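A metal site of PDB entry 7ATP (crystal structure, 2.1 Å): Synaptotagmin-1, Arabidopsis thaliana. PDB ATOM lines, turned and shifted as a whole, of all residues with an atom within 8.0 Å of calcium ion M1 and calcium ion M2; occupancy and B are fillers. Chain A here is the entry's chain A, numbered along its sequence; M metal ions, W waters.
Calcium ion M2 is bound by the side-chain carboxylate (OE2) of Glu 88 (2.2 Å), the side-chain carboxylate (OE1) of Glu 82 (2.2 Å), the side-chain carboxylate (OD1) of Asp 24 (2.3 Å), water W1 (2.4 Å), the backbone carbonyl oxygen (O) of Lys 23 (2.5 Å), the side-chain carboxylate (OD2) of Asp 80 (2.5 Å) and the side-chain carboxylate (OE2) of Glu 82 (2.8 Å).
Of the 24 residues printed, 5 come within 4 Å of calcium ion M1. The nearest printed residue that does not touch calcium ion M1 is Ala 29 (4.6 Å).
O of Gly 28 is in hydrogen-bond range of N of Lys 23, at 2.6 Å. OD1 of Asp 30 is in hydrogen-bond range of N of Lys 52 (2.9 Å). N of Asp 80 lies close to SD of Met 90 (3.7 Å).
Calcium ion M1 is bound by OD2 of Asp 24 (2.3 Å), water W2 (2.3 Å), OD1 of Asp 80 (2.3 Å), OE2 of Glu 82 (2.4 Å), OD2 of Asp 30 (2.4 Å), OD1 of Asp 24 (2.5 Å) and O of Trp 81 (2.6 Å). Calcium ion M1 has seven donor atoms within binding distance. Slightly farther from calcium ion M1 lies the side-chain carboxylate (OD2) of Asp 80 (3.0 Å).
Of the 24 residues printed, 5 come within 4 Å of calcium ion M2.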
ATOM      1  N   LYS A  22     -16.027  22.499 -33.996  1.00  0.00           N
ATOM      2  CA  LYS A  22     -16.674  22.439 -32.697  1.00  0.00           C
ATOM      3  C   LYS A  22     -15.903  21.466 -31.813  1.00  0.00           C
ATOM      4  O   LYS A  22     -15.590  20.350 -32.222  1.00  0.00           O
ATOM      5  CB  LYS A  22     -18.121  21.998 -32.841  1.00  0.00           C
ATOM      6  CG  LYS A  22     -19.031  23.067 -33.428  1.00  0.00           C
ATOM      7  CD  LYS A  22     -20.485  22.583 -33.524  1.00  0.00           C
ATOM      8  CE  LYS A  22     -21.438  23.706 -33.955  1.00  0.00           C
ATOM      9  NZ  LYS A  22     -22.875  23.315 -33.833  1.00  0.00           N
ATOM     10  N   LYS A  23     -15.559  21.916 -30.619  1.00  0.00           N
ATOM     11  CA  LYS A  23     -14.813  21.060 -29.720  1.00  0.00           C
ATOM     12  C   LYS A  23     -15.407  21.027 -28.325  1.00  0.00           C
ATOM     13  O   LYS A  23     -14.848  20.366 -27.435  1.00  0.00           O
ATOM     14  CB  LYS A  23     -13.347  21.500 -29.676  1.00  0.00           C
ATOM     15  CG  LYS A  23     -12.600  21.211 -30.965  1.00  0.00           C
ATOM     16  CD  LYS A  23     -11.308  20.440 -30.693  1.00  0.00           C
ATOM     17  CE  LYS A  23     -11.155  19.232 -31.607  1.00  0.00           C
ATOM     18  NZ  LYS A  23     -11.501  19.547 -33.017  1.00  0.00           N
ATOM     19  N   ASP A  24     -16.533  21.696 -28.099  1.00  0.00           N
ATOM     20  CA  ASP A  24     -17.186  21.702 -26.804  1.00  0.00           C
ATOM     21  C   ASP A  24     -18.613  21.230 -26.957  1.00  0.00           C
ATOM     22  O   ASP A  24     -19.232  21.377 -28.014  1.00  0.00           O
ATOM     23  CB  ASP A  24     -17.200  23.085 -26.160  1.00  0.00           C
ATOM     24  CG  ASP A  24     -15.871  23.464 -25.556  1.00  0.00           C
ATOM     25  OD1 ASP A  24     -15.111  22.523 -25.232  1.00  0.00           O
ATOM     26  OD2 ASP A  24     -15.601  24.681 -25.408  1.00  0.00           O
ATOM     27  N   LEU A  25     -19.146  20.693 -25.854  1.00  0.00           N
ATOM     28  CA  LEU A  25     -20.542  20.274 -25.818  1.00  0.00           C
ATOM     29  C   LEU A  25     -21.468  21.402 -26.259  1.00  0.00           C
ATOM     30  O   LEU A  25     -22.440  21.170 -26.980  1.00  0.00           O
ATOM     31  CB  LEU A  25     -20.908  19.810 -24.417  1.00  0.00           C
ATOM     32  CG  LEU A  25     -22.145  18.933 -24.330  1.00  0.00           C
ATOM     33  CD1 LEU A  25     -21.999  17.762 -25.291  1.00  0.00           C
ATOM     34  CD2 LEU A  25     -22.299  18.454 -22.892  1.00  0.00           C
ATOM     35  N   MET A  26     -21.171  22.632 -25.850  1.00  0.00           N
ATOM     36  CA  MET A  26     -21.925  23.793 -26.290  1.00  0.00           C
ATOM     37  C   MET A  26     -21.046  25.032 -26.237  1.00  0.00           C
ATOM     38  O   MET A  26     -20.206  25.173 -25.326  1.00  0.00           O
ATOM     39  CB  MET A  26     -23.190  24.004 -25.462  1.00  0.00           C
ATOM     40  CG  MET A  26     -22.966  24.565 -24.086  1.00  0.00           C
ATOM     41  SD  MET A  26     -24.472  24.411 -23.104  1.00  0.00           S
ATOM     42  CE  MET A  26     -24.347  22.724 -22.509  1.00  0.00           C
ATOM     43  N   GLY A  27     -21.237  25.913 -27.208  1.00  0.00           N
ATOM     44  CA  GLY A  27     -20.487  27.133 -27.329  1.00  0.00           C
ATOM     45  C   GLY A  27     -19.430  27.114 -28.408  1.00  0.00           C
ATOM     46  O   GLY A  27     -18.827  28.163 -28.688  1.00  0.00           O
ATOM     47  N   GLY A  28     -19.180  25.961 -29.027  1.00  0.00           N
ATOM     48  CA  GLY A  28     -18.224  25.840 -30.099  1.00  0.00           C
ATOM     49  C   GLY A  28     -16.878  25.344 -29.607  1.00  0.00           C
ATOM     50  O   GLY A  28     -16.559  24.153 -29.725  1.00  0.00           O
ATOM     51  N   ALA A  29     -16.092  26.274 -29.065  1.00  0.00           N
ATOM     52  CA  ALA A  29     -14.746  26.046 -28.571  1.00  0.00           C
ATOM     53  C   ALA A  29     -14.313  27.339 -27.903  1.00  0.00           C
ATOM     54  O   ALA A  29     -14.956  28.385 -28.033  1.00  0.00           O
ATOM     55  CB  ALA A  29     -13.771  25.655 -29.691  1.00  0.00           C
ATOM     56  N   ASP A  30     -13.205  27.276 -27.180  1.00  0.00           N
ATOM     57  CA  ASP A  30     -12.617  28.440 -26.525  1.00  0.00           C
ATOM     58  C   ASP A  30     -11.197  28.568 -27.028  1.00  0.00           C
ATOM     59  O   ASP A  30     -10.246  28.223 -26.308  1.00  0.00           O
ATOM     60  CB  ASP A  30     -12.694  28.271 -25.009  1.00  0.00           C
ATOM     61  CG  ASP A  30     -14.066  27.773 -24.543  1.00  0.00           C
ATOM     62  OD1 ASP A  30     -15.056  28.529 -24.675  1.00  0.00           O
ATOM     63  OD2 ASP A  30     -14.212  26.620 -24.064  1.00  0.00           O
ATOM     64  N   PRO A  31     -11.010  29.025 -28.268  1.00  0.00           N
ATOM     65  CA  PRO A  31      -9.686  28.952 -28.878  1.00  0.00           C
ATOM     66  C   PRO A  31      -8.733  29.946 -28.257  1.00  0.00           C
ATOM     67  O   PRO A  31      -9.124  31.017 -27.816  1.00  0.00           O
ATOM     68  CB  PRO A  31      -9.949  29.272 -30.352  1.00  0.00           C
ATOM     69  CG  PRO A  31     -11.208  30.023 -30.347  1.00  0.00           C
ATOM     70  CD  PRO A  31     -12.032  29.405 -29.248  1.00  0.00           C
ATOM     71  N   VAL A  49      -7.810  33.889 -24.565  1.00  0.00           N
ATOM     72  CA  VAL A  49      -8.824  32.886 -24.889  1.00  0.00           C
ATOM     73  C   VAL A  49     -10.077  33.596 -25.366  1.00  0.00           C
ATOM     74  O   VAL A  49     -10.536  34.555 -24.741  1.00  0.00           O
ATOM     75  CB  VAL A  49      -9.170  32.026 -23.656  1.00  0.00           C
ATOM     76  CG1 VAL A  49     -10.334  31.072 -24.017  1.00  0.00           C
ATOM     77  CG2 VAL A  49      -7.993  31.266 -23.209  1.00  0.00           C
ATOM     78  N   HIS A  51     -13.578  32.861 -25.526  1.00  0.00           N
ATOM     79  CA  HIS A  51     -14.577  31.884 -25.111  1.00  0.00           C
ATOM     80  C   HIS A  51     -15.713  31.792 -26.108  1.00  0.00           C
ATOM     81  O   HIS A  51     -16.184  32.796 -26.640  1.00  0.00           O
ATOM     82  CB  HIS A  51     -15.153  32.261 -23.763  1.00  0.00           C
ATOM     83  CG  HIS A  51     -14.157  32.236 -22.676  1.00  0.00           C
ATOM     84  ND1 HIS A  51     -13.668  31.068 -22.136  1.00  0.00           N
ATOM     85  CD2 HIS A  51     -13.553  33.243 -22.005  1.00  0.00           C
ATOM     86  CE1 HIS A  51     -12.788  31.357 -21.194  1.00  0.00           C
ATOM     87  NE2 HIS A  51     -12.696  32.667 -21.100  1.00  0.00           N
ATOM     88  N   LYS A  52     -16.189  30.564 -26.325  1.00  0.00           N
ATOM     89  CA  LYS A  52     -17.422  30.322 -27.061  1.00  0.00           C
ATOM     90  C   LYS A  52     -17.400  31.037 -28.411  1.00  0.00           C
ATOM     91  O   LYS A  52     -18.316  31.770 -28.784  1.00  0.00           O
ATOM     92  CB  LYS A  52     -18.626  30.723 -26.204  1.00  0.00           C
ATOM     93  CG  LYS A  52     -18.712  29.852 -24.912  1.00  0.00           C
ATOM     94  CD  LYS A  52     -19.873  30.239 -24.007  1.00  0.00           C
ATOM     95  CE  LYS A  52     -19.786  29.502 -22.665  1.00  0.00           C
ATOM     96  NZ  LYS A  52     -19.525  28.056 -22.903  1.00  0.00           N
ATOM     97  N   TYR A  79      -5.437  25.845 -29.656  1.00  0.00           N
ATOM     98  CA  TYR A  79      -5.977  25.006 -28.608  1.00  0.00           C
ATOM     99  C   TYR A  79      -7.329  25.527 -28.154  1.00  0.00           C
ATOM    100  O   TYR A  79      -7.630  26.731 -28.228  1.00  0.00           O
ATOM    101  CB  TYR A  79      -5.050  24.943 -27.399  1.00  0.00           C
ATOM    102  CG  TYR A  79      -3.737  24.238 -27.616  1.00  0.00           C
ATOM    103  CD1 TYR A  79      -3.629  22.860 -27.457  1.00  0.00           C
ATOM    104  CD2 TYR A  79      -2.580  24.956 -27.908  1.00  0.00           C
ATOM    105  CE1 TYR A  79      -2.413  22.213 -27.626  1.00  0.00           C
ATOM    106  CE2 TYR A  79      -1.361  24.322 -28.074  1.00  0.00           C
ATOM    107  CZ  TYR A  79      -1.278  22.944 -27.934  1.00  0.00           C
ATOM    108  OH  TYR A  79      -0.056  22.318 -28.106  1.00  0.00           O
ATOM    109  N   ASP A  80      -8.147  24.600 -27.670  1.00  0.00           N
ATOM    110  CA  ASP A  80      -9.437  24.899 -27.055  1.00  0.00           C
ATOM    111  C   ASP A  80      -9.305  24.785 -25.534  1.00  0.00           C
ATOM    112  O   ASP A  80      -9.154  23.681 -24.997  1.00  0.00           O
ATOM    113  CB  ASP A  80     -10.494  23.966 -27.608  1.00  0.00           C
ATOM    114  CG  ASP A  80     -11.733  23.883 -26.726  1.00  0.00           C
ATOM    115  OD1 ASP A  80     -12.191  24.932 -26.217  1.00  0.00           O
ATOM    116  OD2 ASP A  80     -12.258  22.779 -26.580  1.00  0.00           O
ATOM    117  N   TRP A  81      -9.362  25.923 -24.855  1.00  0.00           N
ATOM    118  CA  TRP A  81      -9.229  25.929 -23.408  1.00  0.00           C
ATOM    119  C   TRP A  81     -10.349  25.111 -22.784  1.00  0.00           C
ATOM    120  O   TRP A  81     -11.492  25.146 -23.253  1.00  0.00           O
ATOM    121  CB  TRP A  81      -9.265  27.376 -22.916  1.00  0.00           C
ATOM    122  CG  TRP A  81      -9.387  27.611 -21.405  1.00  0.00           C
ATOM    123  CD1 TRP A  81      -8.364  27.824 -20.523  1.00  0.00           C
ATOM    124  CD2 TRP A  81     -10.604  27.778 -20.661  1.00  0.00           C
ATOM    125  NE1 TRP A  81      -8.877  28.099 -19.273  1.00  0.00           N
ATOM    126  CE2 TRP A  81     -10.248  28.075 -19.336  1.00  0.00           C
ATOM    127  CE3 TRP A  81     -11.940  27.741 -20.997  1.00  0.00           C
ATOM    128  CZ2 TRP A  81     -11.196  28.270 -18.324  1.00  0.00           C
ATOM    129  CZ3 TRP A  81     -12.891  27.959 -19.992  1.00  0.00           C
ATOM    130  CH2 TRP A  81     -12.508  28.210 -18.675  1.00  0.00           C
ATOM    131  N   GLU A  82     -10.032  24.348 -21.762  1.00  0.00           N
ATOM    132  CA  GLU A  82     -11.039  23.554 -21.078  1.00  0.00           C
ATOM    133  C   GLU A  82     -11.222  24.044 -19.662  1.00  0.00           C
ATOM    134  O   GLU A  82     -10.274  24.506 -19.008  1.00  0.00           O
ATOM    135  CB  GLU A  82     -10.683  22.062 -21.069  1.00  0.00           C
ATOM    136  CG  GLU A  82     -10.470  21.492 -22.463  1.00  0.00           C
ATOM    137  CD  GLU A  82     -11.740  21.482 -23.310  1.00  0.00           C
ATOM    138  OE1 GLU A  82     -12.161  20.383 -23.753  1.00  0.00           O
ATOM    139  OE2 GLU A  82     -12.334  22.575 -23.508  1.00  0.00           O
ATOM    140  N   GLN A  83     -12.468  23.954 -19.188  1.00  0.00           N
ATOM    141  CA  GLN A  83     -12.735  24.320 -17.821  1.00  0.00           C
ATOM    142  C   GLN A  83     -12.103  23.328 -16.876  1.00  0.00           C
ATOM    143  O   GLN A  83     -11.735  23.685 -15.758  1.00  0.00           O
ATOM    144  CB  GLN A  83     -14.225  24.419 -17.592  1.00  0.00           C
ATOM    145  CG  GLN A  83     -14.814  25.474 -18.473  1.00  0.00           C
ATOM    146  CD  GLN A  83     -16.183  25.864 -18.047  1.00  0.00           C
ATOM    147  OE1 GLN A  83     -16.834  25.100 -17.327  1.00  0.00           O
ATOM    148  NE2 GLN A  83     -16.631  27.063 -18.457  1.00  0.00           N
ATOM    149  N   VAL A  84     -11.908  22.098 -17.324  1.00  0.00           N
ATOM    150  CA  VAL A  84     -11.300  21.078 -16.493  1.00  0.00           C
ATOM    151  C   VAL A  84     -10.261  20.351 -17.329  1.00  0.00           C
ATOM    152  O   VAL A  84     -10.549  19.933 -18.457  1.00  0.00           O
ATOM    153  CB  VAL A  84     -12.348  20.113 -15.928  1.00  0.00           C
ATOM    154  CG1 VAL A  84     -11.649  19.005 -15.174  1.00  0.00           C
ATOM    155  CG2 VAL A  84     -13.298  20.867 -15.027  1.00  0.00           C
ATOM    156  N   ASN A  86      -6.594  19.885 -19.240  1.00  0.00           N
ATOM    157  CA  ASN A  86      -5.728  20.677 -20.064  1.00  0.00           C
ATOM    158  C   ASN A  86      -6.416  21.060 -21.362  1.00  0.00           C
ATOM    159  O   ASN A  86      -7.349  20.374 -21.799  1.00  0.00           O
ATOM    160  CB  ASN A  86      -4.434  19.904 -20.373  1.00  0.00           C
ATOM    161  CG  ASN A  86      -3.386  20.080 -19.283  1.00  0.00           C
ATOM    162  OD1 ASN A  86      -3.348  21.120 -18.618  1.00  0.00           O
ATOM    163  ND2 ASN A  86      -2.536  19.069 -19.104  1.00  0.00           N
ATOM    164  N   PRO A  87      -6.005  22.153 -21.978  1.00  0.00           N
ATOM    165  CA  PRO A  87      -6.575  22.533 -23.271  1.00  0.00           C
ATOM    166  C   PRO A  87      -6.407  21.382 -24.244  1.00  0.00           C
ATOM    167  O   PRO A  87      -5.493  20.575 -24.088  1.00  0.00           O
ATOM    168  CB  PRO A  87      -5.746  23.758 -23.684  1.00  0.00           C
ATOM    169  CG  PRO A  87      -5.298  24.335 -22.385  1.00  0.00           C
ATOM    170  CD  PRO A  87      -4.978  23.123 -21.544  1.00  0.00           C
ATOM    171  N   GLU A  88      -7.317  21.281 -25.205  1.00  0.00           N
ATOM    172  CA  GLU A  88      -7.221  20.257 -26.235  1.00  0.00           C
ATOM    173  C   GLU A  88      -6.821  20.878 -27.559  1.00  0.00           C
ATOM    174  O   GLU A  88      -7.407  21.874 -27.980  1.00  0.00           O
ATOM    175  CB  GLU A  88      -8.533  19.487 -26.389  1.00  0.00           C
ATOM    176  CG  GLU A  88      -9.738  20.272 -26.784  1.00  0.00           C
ATOM    177  CD  GLU A  88     -10.932  19.369 -27.076  1.00  0.00           C
ATOM    178  OE1 GLU A  88     -10.779  18.409 -27.867  1.00  0.00           O
ATOM    179  OE2 GLU A  88     -12.018  19.616 -26.500  1.00  0.00           O
ATOM    180  N   LYS A  89      -5.812  20.281 -28.180  1.00  0.00           N
ATOM    181  CA  LYS A  89      -5.327  20.753 -29.465  1.00  0.00           C
ATOM    182  C   LYS A  89      -6.481  20.844 -30.460  1.00  0.00           C
ATOM    183  O   LYS A  89      -7.406  20.018 -30.433  1.00  0.00           O
ATOM    184  CB  LYS A  89      -4.248  19.821 -30.000  1.00  0.00           C
ATOM    185  CG  LYS A  89      -3.645  20.240 -31.331  1.00  0.00           C
ATOM    186  CD  LYS A  89      -2.742  21.467 -31.183  1.00  0.00           C
ATOM    187  CE  LYS A  89      -1.312  21.149 -31.615  1.00  0.00           C
ATOM    188  NZ  LYS A  89      -0.753  19.992 -30.841  1.00  0.00           N
ATOM    189  N   MET A  90      -6.438  21.861 -31.315  1.00  0.00           N
ATOM    190  CA  MET A  90      -7.372  21.989 -32.420  1.00  0.00           C
ATOM    191  C   MET A  90      -6.688  21.982 -33.787  1.00  0.00           C
ATOM    192  O   MET A  90      -7.379  22.055 -34.813  1.00  0.00           O
ATOM    193  CB  MET A  90      -8.201  23.271 -32.277  1.00  0.00           C
ATOM    194  CG  MET A  90      -9.109  23.260 -31.096  1.00  0.00           C
ATOM    195  SD  MET A  90      -9.852  24.862 -30.947  1.00  0.00           S
ATOM    196  CE  MET A  90     -11.148  24.807 -32.175  1.00  0.00           C
HETATM  197 CA    CA M   1     -13.598  24.327 -24.435  1.00  0.00          CA
HETATM  198 CA    CA M   2     -13.483  20.946 -25.477  1.00  0.00          CA
HETATM  199  O   HOH W   1     -14.981  19.595 -24.247  1.00  0.00           O
HETATM  200  O   HOH W   2     -14.811  24.253 -22.533  1.00  0.00           O
